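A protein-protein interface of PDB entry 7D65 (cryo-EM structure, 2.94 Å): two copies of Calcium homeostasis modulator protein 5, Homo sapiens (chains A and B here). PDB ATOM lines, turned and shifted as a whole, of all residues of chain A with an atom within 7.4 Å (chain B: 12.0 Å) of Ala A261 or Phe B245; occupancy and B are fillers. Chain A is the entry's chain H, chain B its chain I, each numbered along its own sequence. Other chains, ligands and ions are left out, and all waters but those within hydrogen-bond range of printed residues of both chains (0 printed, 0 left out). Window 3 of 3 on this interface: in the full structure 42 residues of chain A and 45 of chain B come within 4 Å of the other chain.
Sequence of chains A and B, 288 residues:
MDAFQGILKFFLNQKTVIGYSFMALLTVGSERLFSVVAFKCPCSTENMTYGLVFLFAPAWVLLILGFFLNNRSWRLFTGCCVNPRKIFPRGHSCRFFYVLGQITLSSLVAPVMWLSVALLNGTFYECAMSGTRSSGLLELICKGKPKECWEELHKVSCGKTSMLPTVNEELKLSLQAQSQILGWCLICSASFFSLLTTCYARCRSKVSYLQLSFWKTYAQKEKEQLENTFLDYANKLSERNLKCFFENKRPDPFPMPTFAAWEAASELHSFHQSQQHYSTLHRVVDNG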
ATOM      1  N   LEU A 226      19.945  -1.694  20.560  1.00  0.00           N
ATOM      2  CA  LEU A 226      18.939  -0.813  19.987  1.00  0.00           C
ATOM      3  C   LEU A 226      18.513   0.263  20.968  1.00  0.00           C
ATOM      4  O   LEU A 226      18.188   1.374  20.554  1.00  0.00           O
ATOM      5  CB  LEU A 226      17.728  -1.621  19.549  1.00  0.00           C
ATOM      6  CG  LEU A 226      16.923  -1.162  18.348  1.00  0.00           C
ATOM      7  CD1 LEU A 226      17.815  -0.946  17.164  1.00  0.00           C
ATOM      8  CD2 LEU A 226      15.915  -2.211  18.041  1.00  0.00           C
ATOM      9  N   PHE A 230      19.190   4.269  20.003  1.00  0.00           N
ATOM     10  CA  PHE A 230      18.033   5.153  20.068  1.00  0.00           C
ATOM     11  C   PHE A 230      18.263   6.307  21.020  1.00  0.00           C
ATOM     12  O   PHE A 230      17.730   7.395  20.807  1.00  0.00           O
ATOM     13  CB  PHE A 230      16.796   4.392  20.524  1.00  0.00           C
ATOM     14  CG  PHE A 230      16.121   3.620  19.448  1.00  0.00           C
ATOM     15  CD1 PHE A 230      16.550   3.689  18.140  1.00  0.00           C
ATOM     16  CD2 PHE A 230      15.045   2.827  19.746  1.00  0.00           C
ATOM     17  CE1 PHE A 230      15.920   2.977  17.162  1.00  0.00           C
ATOM     18  CE2 PHE A 230      14.412   2.120  18.768  1.00  0.00           C
ATOM     19  CZ  PHE A 230      14.854   2.195  17.476  1.00  0.00           C
ATOM     20  N   TYR A 233      21.013   8.832  19.173  1.00  0.00           N
ATOM     21  CA  TYR A 233      20.483   9.659  18.104  1.00  0.00           C
ATOM     22  C   TYR A 233      19.342  10.544  18.567  1.00  0.00           C
ATOM     23  O   TYR A 233      18.854  11.354  17.779  1.00  0.00           O
ATOM     24  CB  TYR A 233      19.999   8.789  16.948  1.00  0.00           C
ATOM     25  CG  TYR A 233      21.080   8.355  16.004  1.00  0.00           C
ATOM     26  CD1 TYR A 233      21.132   8.842  14.712  1.00  0.00           C
ATOM     27  CD2 TYR A 233      22.044   7.452  16.400  1.00  0.00           C
ATOM     28  CE1 TYR A 233      22.117   8.444  13.843  1.00  0.00           C
ATOM     29  CE2 TYR A 233      23.033   7.048  15.543  1.00  0.00           C
ATOM     30  CZ  TYR A 233      23.066   7.545  14.268  1.00  0.00           C
ATOM     31  OH  TYR A 233      24.061   7.131  13.413  1.00  0.00           O
ATOM     32  N   MET A 256      18.577  10.370   8.891  1.00  0.00           N
ATOM     33  CA  MET A 256      17.732   9.353   9.488  1.00  0.00           C
ATOM     34  C   MET A 256      17.219   8.436   8.388  1.00  0.00           C
ATOM     35  O   MET A 256      17.166   8.851   7.227  1.00  0.00           O
ATOM     36  CB  MET A 256      16.546   9.991  10.220  1.00  0.00           C
ATOM     37  CG  MET A 256      16.919  10.766  11.459  1.00  0.00           C
ATOM     38  SD  MET A 256      17.354   9.691  12.824  1.00  0.00           S
ATOM     39  CE  MET A 256      15.844   8.768  12.971  1.00  0.00           C
ATOM     40  N   PRO A 257      16.866   7.186   8.698  1.00  0.00           N
ATOM     41  CA  PRO A 257      16.361   6.287   7.654  1.00  0.00           C
ATOM     42  C   PRO A 257      14.996   6.709   7.139  1.00  0.00           C
ATOM     43  O   PRO A 257      14.258   7.458   7.777  1.00  0.00           O
ATOM     44  CB  PRO A 257      16.294   4.923   8.349  1.00  0.00           C
ATOM     45  CG  PRO A 257      16.444   5.194   9.776  1.00  0.00           C
ATOM     46  CD  PRO A 257      17.230   6.439   9.910  1.00  0.00           C
ATOM     47  N   THR A 258      14.677   6.225   5.945  1.00  0.00           N
ATOM     48  CA  THR A 258      13.418   6.563   5.309  1.00  0.00           C
ATOM     49  C   THR A 258      12.262   5.851   5.998  1.00  0.00           C
ATOM     50  O   THR A 258      12.450   4.956   6.818  1.00  0.00           O
ATOM     51  CB  THR A 258      13.451   6.192   3.829  1.00  0.00           C
ATOM     52  OG1 THR A 258      14.077   4.917   3.674  1.00  0.00           O
ATOM     53  CG2 THR A 258      14.222   7.215   3.040  1.00  0.00           C
ATOM     54  N   PHE A 259      11.044   6.263   5.657  1.00  0.00           N
ATOM     55  CA  PHE A 259       9.871   5.590   6.197  1.00  0.00           C
ATOM     56  C   PHE A 259       9.702   4.205   5.597  1.00  0.00           C
ATOM     57  O   PHE A 259       9.154   3.313   6.249  1.00  0.00           O
ATOM     58  CB  PHE A 259       8.620   6.430   5.953  1.00  0.00           C
ATOM     59  CG  PHE A 259       7.359   5.800   6.453  1.00  0.00           C
ATOM     60  CD1 PHE A 259       7.149   5.621   7.807  1.00  0.00           C
ATOM     61  CD2 PHE A 259       6.391   5.372   5.569  1.00  0.00           C
ATOM     62  CE1 PHE A 259       5.995   5.036   8.265  1.00  0.00           C
ATOM     63  CE2 PHE A 259       5.238   4.787   6.024  1.00  0.00           C
ATOM     64  CZ  PHE A 259       5.040   4.621   7.373  1.00  0.00           C
ATOM     65  N   ALA A 260      10.182   3.995   4.374  1.00  0.00           N
ATOM     66  CA  ALA A 260      10.077   2.682   3.757  1.00  0.00           C
ATOM     67  C   ALA A 260      11.050   1.677   4.353  1.00  0.00           C
ATOM     68  O   ALA A 260      10.856   0.475   4.171  1.00  0.00           O
ATOM     69  CB  ALA A 260      10.297   2.792   2.253  1.00  0.00           C
ATOM     70  N   ALA A 261      12.082   2.134   5.061  1.00  0.00           N
ATOM     71  CA  ALA A 261      12.997   1.228   5.736  1.00  0.00           C
ATOM     72  C   ALA A 261      12.723   1.092   7.223  1.00  0.00           C
ATOM     73  O   ALA A 261      13.215   0.144   7.838  1.00  0.00           O
ATOM     74  CB  ALA A 261      14.442   1.680   5.538  1.00  0.00           C
ATOM     75  N   TRP A 262      11.975   2.020   7.821  1.00  0.00           N
ATOM     76  CA  TRP A 262      11.466   1.796   9.165  1.00  0.00           C
ATOM     77  C   TRP A 262      10.367   0.746   9.152  1.00  0.00           C
ATOM     78  O   TRP A 262      10.192   0.020  10.133  1.00  0.00           O
ATOM     79  CB  TRP A 262      10.915   3.094   9.757  1.00  0.00           C
ATOM     80  CG  TRP A 262      11.886   4.082  10.371  1.00  0.00           C
ATOM     81  CD1 TRP A 262      12.207   5.302   9.880  1.00  0.00           C
ATOM     82  CD2 TRP A 262      12.573   3.965  11.619  1.00  0.00           C
ATOM     83  NE1 TRP A 262      13.077   5.937  10.715  1.00  0.00           N
ATOM     84  CE2 TRP A 262      13.316   5.138  11.795  1.00  0.00           C
ATOM     85  CE3 TRP A 262      12.647   2.975  12.596  1.00  0.00           C
ATOM     86  CZ2 TRP A 262      14.119   5.351  12.902  1.00  0.00           C
ATOM     87  CZ3 TRP A 262      13.446   3.190  13.693  1.00  0.00           C
ATOM     88  CH2 TRP A 262      14.171   4.365  13.837  1.00  0.00           C
ATOM     89  N   GLU A 263       9.610   0.666   8.057  1.00  0.00           N
ATOM     90  CA  GLU A 263       8.517  -0.292   7.934  1.00  0.00           C
ATOM     91  C   GLU A 263       9.002  -1.694   7.611  1.00  0.00           C
ATOM     92  O   GLU A 263       8.375  -2.669   8.031  1.00  0.00           O
ATOM     93  CB  GLU A 263       7.551   0.156   6.845  1.00  0.00           C
ATOM     94  CG  GLU A 263       6.668   1.299   7.235  1.00  0.00           C
ATOM     95  CD  GLU A 263       5.380   0.843   7.875  1.00  0.00           C
ATOM     96  OE1 GLU A 263       4.737  -0.064   7.315  1.00  0.00           O
ATOM     97  OE2 GLU A 263       5.012   1.374   8.944  1.00  0.00           O
ATOM     98  N   ALA A 264      10.096  -1.818   6.858  1.00  0.00           N
ATOM     99  CA  ALA A 264      10.576  -3.133   6.460  1.00  0.00           C
ATOM    100  C   ALA A 264      11.264  -3.854   7.606  1.00  0.00           C
ATOM    101  O   ALA A 264      11.189  -5.080   7.690  1.00  0.00           O
ATOM    102  CB  ALA A 264      11.521  -3.012   5.272  1.00  0.00           C
ATOM    103  N   ALA A 265      11.920  -3.125   8.501  1.00  0.00           N
ATOM    104  CA  ALA A 265      12.608  -3.723   9.636  1.00  0.00           C
ATOM    105  C   ALA A 265      11.697  -3.966  10.826  1.00  0.00           C
ATOM    106  O   ALA A 265      12.194  -4.228  11.921  1.00  0.00           O
ATOM    107  CB  ALA A 265      13.776  -2.846  10.069  1.00  0.00           C
ATOM    108  N   SER A 266      10.382  -3.883  10.639  1.00  0.00           N
ATOM    109  CA  SER A 266       9.408  -4.140  11.690  1.00  0.00           C
ATOM    110  C   SER A 266       8.494  -5.305  11.343  1.00  0.00           C
ATOM    111  O   SER A 266       7.435  -5.451  11.950  1.00  0.00           O
ATOM    112  CB  SER A 266       8.566  -2.897  11.960  1.00  0.00           C
ATOM    113  OG  SER A 266       9.275  -1.951  12.731  1.00  0.00           O
ATOM    114  N   LEU A 281      15.957  -7.387  10.942  1.00  0.00           N
ATOM    115  CA  LEU A 281      16.895  -6.304  10.707  1.00  0.00           C
ATOM    116  C   LEU A 281      18.181  -6.805  10.081  1.00  0.00           C
ATOM    117  O   LEU A 281      18.860  -6.052   9.383  1.00  0.00           O
ATOM    118  CB  LEU A 281      17.208  -5.586  12.018  1.00  0.00           C
ATOM    119  CG  LEU A 281      17.971  -4.267  11.995  1.00  0.00           C
ATOM    120  CD1 LEU A 281      17.449  -3.399  10.908  1.00  0.00           C
ATOM    121  CD2 LEU A 281      17.792  -3.581  13.302  1.00  0.00           C
ATOM    122  N   VAL A 284      17.166  -7.050   6.194  1.00  0.00           N
ATOM    123  CA  VAL A 284      17.120  -5.815   5.414  1.00  0.00           C
ATOM    124  C   VAL A 284      18.481  -5.171   5.233  1.00  0.00           C
ATOM    125  O   VAL A 284      18.617  -4.267   4.404  1.00  0.00           O
ATOM    126  CB  VAL A 284      16.175  -4.775   6.044  1.00  0.00           C
ATOM    127  CG1 VAL A 284      14.801  -5.342   6.189  1.00  0.00           C
ATOM    128  CG2 VAL A 284      16.689  -4.344   7.381  1.00  0.00           C
ATOM    129  N   VAL A 285      19.490  -5.602   5.979  1.00  0.00           N
ATOM    130  CA  VAL A 285      20.835  -5.057   5.852  1.00  0.00           C
ATOM    131  C   VAL A 285      21.655  -5.862   4.854  1.00  0.00           C
ATOM    132  O   VAL A 285      22.380  -5.295   4.035  1.00  0.00           O
ATOM    133  CB  VAL A 285      21.484  -5.010   7.252  1.00  0.00           C
ATOM    134  CG1 VAL A 285      22.983  -4.938   7.185  1.00  0.00           C
ATOM    135  CG2 VAL A 285      20.952  -3.837   8.015  1.00  0.00           C
ATOM    136  N   LEU B 237      28.151  -8.859  15.694  1.00  0.00           N
ATOM    137  CA  LEU B 237      27.204  -8.897  14.590  1.00  0.00           C
ATOM    138  C   LEU B 237      26.110  -7.857  14.736  1.00  0.00           C
ATOM    139  O   LEU B 237      25.682  -7.274  13.741  1.00  0.00           O
ATOM    140  CB  LEU B 237      26.578 -10.290  14.469  1.00  0.00           C
ATOM    141  CG  LEU B 237      25.481 -10.524  13.430  1.00  0.00           C
ATOM    142  CD1 LEU B 237      26.011 -10.293  12.045  1.00  0.00           C
ATOM    143  CD2 LEU B 237      24.900 -11.910  13.543  1.00  0.00           C
ATOM    144  N   SER B 238      25.663  -7.589  15.957  1.00  0.00           N
ATOM    145  CA  SER B 238      24.636  -6.580  16.154  1.00  0.00           C
ATOM    146  C   SER B 238      25.187  -5.168  16.028  1.00  0.00           C
ATOM    147  O   SER B 238      24.438  -4.255  15.683  1.00  0.00           O
ATOM    148  CB  SER B 238      23.980  -6.765  17.515  1.00  0.00           C
ATOM    149  OG  SER B 238      24.688  -6.054  18.500  1.00  0.00           O
ATOM    150  N   GLU B 239      26.476  -4.960  16.302  1.00  0.00           N
ATOM    151  CA  GLU B 239      27.086  -3.658  16.052  1.00  0.00           C
ATOM    152  C   GLU B 239      27.196  -3.368  14.566  1.00  0.00           C
ATOM    153  O   GLU B 239      27.130  -2.210  14.155  1.00  0.00           O
ATOM    154  CB  GLU B 239      28.475  -3.590  16.673  1.00  0.00           C
ATOM    155  CG  GLU B 239      28.512  -3.115  18.094  1.00  0.00           C
ATOM    156  CD  GLU B 239      29.822  -3.447  18.775  1.00  0.00           C
ATOM    157  OE1 GLU B 239      30.805  -3.745  18.065  1.00  0.00           O
ATOM    158  OE2 GLU B 239      29.873  -3.405  20.022  1.00  0.00           O
ATOM    159  N   ARG B 240      27.383  -4.403  13.756  1.00  0.00           N
ATOM    160  CA  ARG B 240      27.478  -4.231  12.319  1.00  0.00           C
ATOM    161  C   ARG B 240      26.122  -3.964  11.692  1.00  0.00           C
ATOM    162  O   ARG B 240      26.032  -3.198  10.731  1.00  0.00           O
ATOM    163  CB  ARG B 240      28.111  -5.474  11.704  1.00  0.00           C
ATOM    164  CG  ARG B 240      28.472  -5.357  10.259  1.00  0.00           C
ATOM    165  CD  ARG B 240      28.568  -6.719   9.639  1.00  0.00           C
ATOM    166  NE  ARG B 240      27.253  -7.288   9.411  1.00  0.00           N
ATOM    167  CZ  ARG B 240      26.891  -7.890   8.290  1.00  0.00           C
ATOM    168  NH1 ARG B 240      27.746  -8.004   7.295  1.00  0.00           N
ATOM    169  NH2 ARG B 240      25.671  -8.378   8.161  1.00  0.00           N
ATOM    170  N   ASN B 241      25.059  -4.572  12.217  1.00  0.00           N
ATOM    171  CA  ASN B 241      23.733  -4.401  11.639  1.00  0.00           C
ATOM    172  C   ASN B 241      23.135  -3.044  11.959  1.00  0.00           C
ATOM    173  O   ASN B 241      22.370  -2.509  11.157  1.00  0.00           O
ATOM    174  CB  ASN B 241      22.792  -5.490  12.143  1.00  0.00           C
ATOM    175  CG  ASN B 241      23.069  -6.828  11.527  1.00  0.00           C
ATOM    176  OD1 ASN B 241      23.861  -6.947  10.605  1.00  0.00           O
ATOM    177  ND2 ASN B 241      22.406  -7.848  12.032  1.00  0.00           N
ATOM    178  N   LEU B 242      23.444  -2.482  13.124  1.00  0.00           N
ATOM    179  CA  LEU B 242      22.833  -1.221  13.519  1.00  0.00           C
ATOM    180  C   LEU B 242      23.528  -0.024  12.896  1.00  0.00           C
ATOM    181  O   LEU B 242      22.905   1.024  12.721  1.00  0.00           O
ATOM    182  CB  LEU B 242      22.848  -1.079  15.036  1.00  0.00           C
ATOM    183  CG  LEU B 242      22.005  -2.030  15.870  1.00  0.00           C
ATOM    184  CD1 LEU B 242      21.760  -1.406  17.192  1.00  0.00           C
ATOM    185  CD2 LEU B 242      20.708  -2.332  15.210  1.00  0.00           C
ATOM    186  N   LYS B 243      24.811  -0.146  12.575  1.00  0.00           N
ATOM    187  CA  LYS B 243      25.499   0.946  11.907  1.00  0.00           C
ATOM    188  C   LYS B 243      25.160   1.006  10.430  1.00  0.00           C
ATOM    189  O   LYS B 243      25.182   2.087   9.843  1.00  0.00           O
ATOM    190  CB  LYS B 243      27.007   0.809  12.083  1.00  0.00           C
ATOM    191  CG  LYS B 243      27.487   1.079  13.487  1.00  0.00           C
ATOM    192  CD  LYS B 243      28.985   1.290  13.520  1.00  0.00           C
ATOM    193  CE  LYS B 243      29.732   0.117  12.910  1.00  0.00           C
ATOM    194  NZ  LYS B 243      31.180   0.171  13.236  1.00  0.00           N
ATOM    195  N   CYS B 244      24.857  -0.122   9.812  1.00  0.00           N
ATOM    196  CA  CYS B 244      24.498  -0.124   8.406  1.00  0.00           C
ATOM    197  C   CYS B 244      23.010   0.078   8.186  1.00  0.00           C
ATOM    198  O   CYS B 244      22.559   0.031   7.040  1.00  0.00           O
ATOM    199  CB  CYS B 244      24.950  -1.424   7.748  1.00  0.00           C
ATOM    200  SG  CYS B 244      26.722  -1.694   7.828  1.00  0.00           S
ATOM    201  N   PHE B 245      22.241   0.294   9.250  1.00  0.00           N
ATOM    202  CA  PHE B 245      20.835   0.655   9.140  1.00  0.00           C
ATOM    203  C   PHE B 245      20.606   2.149   9.290  1.00  0.00           C
ATOM    204  O   PHE B 245      19.805   2.725   8.552  1.00  0.00           O
ATOM    205  CB  PHE B 245      20.002  -0.084  10.187  1.00  0.00           C
ATOM    206  CG  PHE B 245      18.537   0.191  10.092  1.00  0.00           C
ATOM    207  CD1 PHE B 245      17.835  -0.145   8.954  1.00  0.00           C
ATOM    208  CD2 PHE B 245      17.859   0.789  11.134  1.00  0.00           C
ATOM    209  CE1 PHE B 245      16.489   0.109   8.858  1.00  0.00           C
ATOM    210  CE2 PHE B 245      16.511   1.048  11.039  1.00  0.00           C
ATOM    211  CZ  PHE B 245      15.831   0.706   9.901  1.00  0.00           C
ATOM    212  N   PHE B 246      21.304   2.792  10.218  1.00  0.00           N
ATOM    213  CA  PHE B 246      21.095   4.212  10.441  1.00  0.00           C
ATOM    214  C   PHE B 246      21.916   5.074   9.500  1.00  0.00           C
ATOM    215  O   PHE B 246      21.542   6.219   9.237  1.00  0.00           O
ATOM    216  CB  PHE B 246      21.421   4.557  11.884  1.00  0.00           C
ATOM    217  CG  PHE B 246      20.331   4.217  12.831  1.00  0.00           C
ATOM    218  CD1 PHE B 246      19.327   5.125  13.099  1.00  0.00           C
ATOM    219  CD2 PHE B 246      20.298   2.983  13.444  1.00  0.00           C
ATOM    220  CE1 PHE B 246      18.314   4.813  13.967  1.00  0.00           C
ATOM    221  CE2 PHE B 246      19.288   2.659  14.308  1.00  0.00           C
ATOM    222  CZ  PHE B 246      18.294   3.575  14.571  1.00  0.00           C
ATOM    223  N   GLU B 247      23.025   4.556   8.990  1.00  0.00           N
ATOM    224  CA  GLU B 247      23.883   5.317   8.095  1.00  0.00           C
ATOM    225  C   GLU B 247      23.619   5.037   6.627  1.00  0.00           C
ATOM    226  O   GLU B 247      24.212   5.712   5.780  1.00  0.00           O
ATOM    227  CB  GLU B 247      25.356   5.036   8.406  1.00  0.00           C
ATOM    228  CG  GLU B 247      25.780   5.492   9.784  1.00  0.00           C
ATOM    229  CD  GLU B 247      27.014   4.784  10.269  1.00  0.00           C
ATOM    230  OE1 GLU B 247      27.492   3.883   9.557  1.00  0.00           O
ATOM    231  OE2 GLU B 247      27.508   5.125  11.360  1.00  0.00           O
ATOM    232  N   ASN B 248      22.744   4.072   6.323  1.00  0.00           N
ATOM    233  CA  ASN B 248      22.370   3.672   4.961  1.00  0.00           C
ATOM    234  C   ASN B 248      23.585   3.249   4.136  1.00  0.00           C
ATOM    235  O   ASN B 248      23.830   3.755   3.041  1.00  0.00           O
ATOM    236  CB  ASN B 248      21.576   4.771   4.252  1.00  0.00           C
ATOM    237  CG  ASN B 248      20.690   4.230   3.157  1.00  0.00           C
ATOM    238  OD1 ASN B 248      20.514   3.020   3.028  1.00  0.00           O
ATOM    239  ND2 ASN B 248      20.124   5.125   2.358  1.00  0.00           N
ATOM    240  N   LYS B 249      24.352   2.309   4.674  1.00  0.00           N
ATOM    241  CA  LYS B 249      25.534   1.778   4.016  1.00  0.00           C
ATOM    242  C   LYS B 249      25.338   0.306   3.686  1.00  0.00           C
ATOM    243  O   LYS B 249      24.356  -0.323   4.081  1.00  0.00           O
ATOM    244  CB  LYS B 249      26.773   1.943   4.898  1.00  0.00           C
ATOM    245  CG  LYS B 249      27.147   3.372   5.219  1.00  0.00           C
ATOM    246  CD  LYS B 249      28.198   3.398   6.305  1.00  0.00           C
ATOM    247  CE  LYS B 249      28.668   4.805   6.597  1.00  0.00           C
ATOM    248  NZ  LYS B 249      29.553   4.852   7.798  1.00  0.00           N
ATOM    249  N   ARG B 250      26.297  -0.236   2.949  1.00  0.00           N
ATOM    250  CA  ARG B 250      26.373  -1.667   2.703  1.00  0.00           C
ATOM    251  C   ARG B 250      27.398  -2.292   3.640  1.00  0.00           C
ATOM    252  O   ARG B 250      28.439  -1.684   3.907  1.00  0.00           O
ATOM    253  CB  ARG B 250      26.767  -1.952   1.254  1.00  0.00           C
ATOM    254  CG  ARG B 250      25.967  -1.183   0.221  1.00  0.00           C
ATOM    255  CD  ARG B 250      24.639  -1.849  -0.097  1.00  0.00           C
ATOM    256  NE  ARG B 250      23.514  -1.214   0.586  1.00  0.00           N
ATOM    257  CZ  ARG B 250      22.846  -0.163   0.115  1.00  0.00           C
ATOM    258  NH1 ARG B 250      23.189   0.380  -1.044  1.00  0.00           N
ATOM    259  NH2 ARG B 250      21.832   0.347   0.800  1.00  0.00           N
ATOM    260  N   PRO B 251      27.148  -3.485   4.170  1.00  0.00           N
ATOM    261  CA  PRO B 251      28.023  -4.043   5.198  1.00  0.00           C
ATOM    262  C   PRO B 251      29.118  -4.943   4.641  1.00  0.00           C
ATOM    263  O   PRO B 251      29.040  -5.464   3.526  1.00  0.00           O
ATOM    264  CB  PRO B 251      27.047  -4.856   6.052  1.00  0.00           C
ATOM    265  CG  PRO B 251      26.055  -5.345   5.066  1.00  0.00           C
ATOM    266  CD  PRO B 251      25.968  -4.336   3.951  1.00  0.00           C
ATOM    267  N   ASP B 252      30.158  -5.118   5.459  1.00  0.00           N
ATOM    268  CA  ASP B 252      31.201  -6.090   5.178  1.00  0.00           C
ATOM    269  C   ASP B 252      30.727  -7.492   5.566  1.00  0.00           C
ATOM    270  O   ASP B 252      30.011  -7.654   6.558  1.00  0.00           O
ATOM    271  CB  ASP B 252      32.474  -5.743   5.943  1.00  0.00           C
ATOM    272  CG  ASP B 252      33.140  -4.491   5.420  1.00  0.00           C
ATOM    273  OD1 ASP B 252      32.627  -3.910   4.441  1.00  0.00           O
ATOM    274  OD2 ASP B 252      34.182  -4.091   5.981  1.00  0.00           O
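NH2 of Arg B240 is in hydrogen-bond range of OD1 of Asn B241 (3.4 Å).
Among the printed residues, pairs that only touch across the chains: Leu A226 with Leu B242 (3.8 Å), Phe A230 with Phe B246 (3.6 Å), Tyr A233 with Phe B246 (3.99 Å), Ala A261 with Phe B245 (3.4 Å), Leu A281 with Leu B242 (3.7 Å), Leu A281 with Phe B245 (3.8 Å), Val A285 with Asn B241 (3.7 Å) and Val A285 with Pro B251 (3.7 Å).
Of the printed residues of chain B, Tyr A233 touches Phe B246.
No residue of chain B comes within 4 Å of Thr A258.
No residue of chain B comes within 4 Å of Phe A259.
Of chain B, only Phe B245 (3.4 Å) comes within 4 Å of Ala A261.
No residue of chain B comes within 4 Å of Trp A262.
Printed residues of chain B within 4 Å of Leu A281: Leu B242 (3.7 Å) and Phe B245 (3.8 Å).
Val A285 touches just these residues of chain B: Asn B241 and Pro B251.
Leu B237 touches none of the printed residues of chain A.
Ser B238 touches none of the printed residues of chain A.
Of the printed residues of chain A, Phe B246 touches Phe A230 (3.6 Å) and Tyr A233 (3.99 Å).
The nearest residue of chain B that does not touch Ala A261 is Asn B248 (6.7 Å).
The nearest residue of chain A that does not touch Phe B245 is Ala A265 (4.1 Å).
Printed residues of chain B that touch a printed residue of chain A: Asn B241, Leu B242, Phe B245, Phe B246 and Pro B251.
Of the 17 printed residues of chain A, 6 touch a printed residue of chain B.
Printed residues of chain A that touch a printed residue of chain B: Leu A226, Phe A230, Tyr A233, Ala A261, Leu A281 and Val A285.
Hydrophobic or aromatic side chains of chain A within 4 Å of the printed part of chain B: Leu A226, Phe A230, Tyr A233, Leu A281 and Val A285.
No position is printed for both chains.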
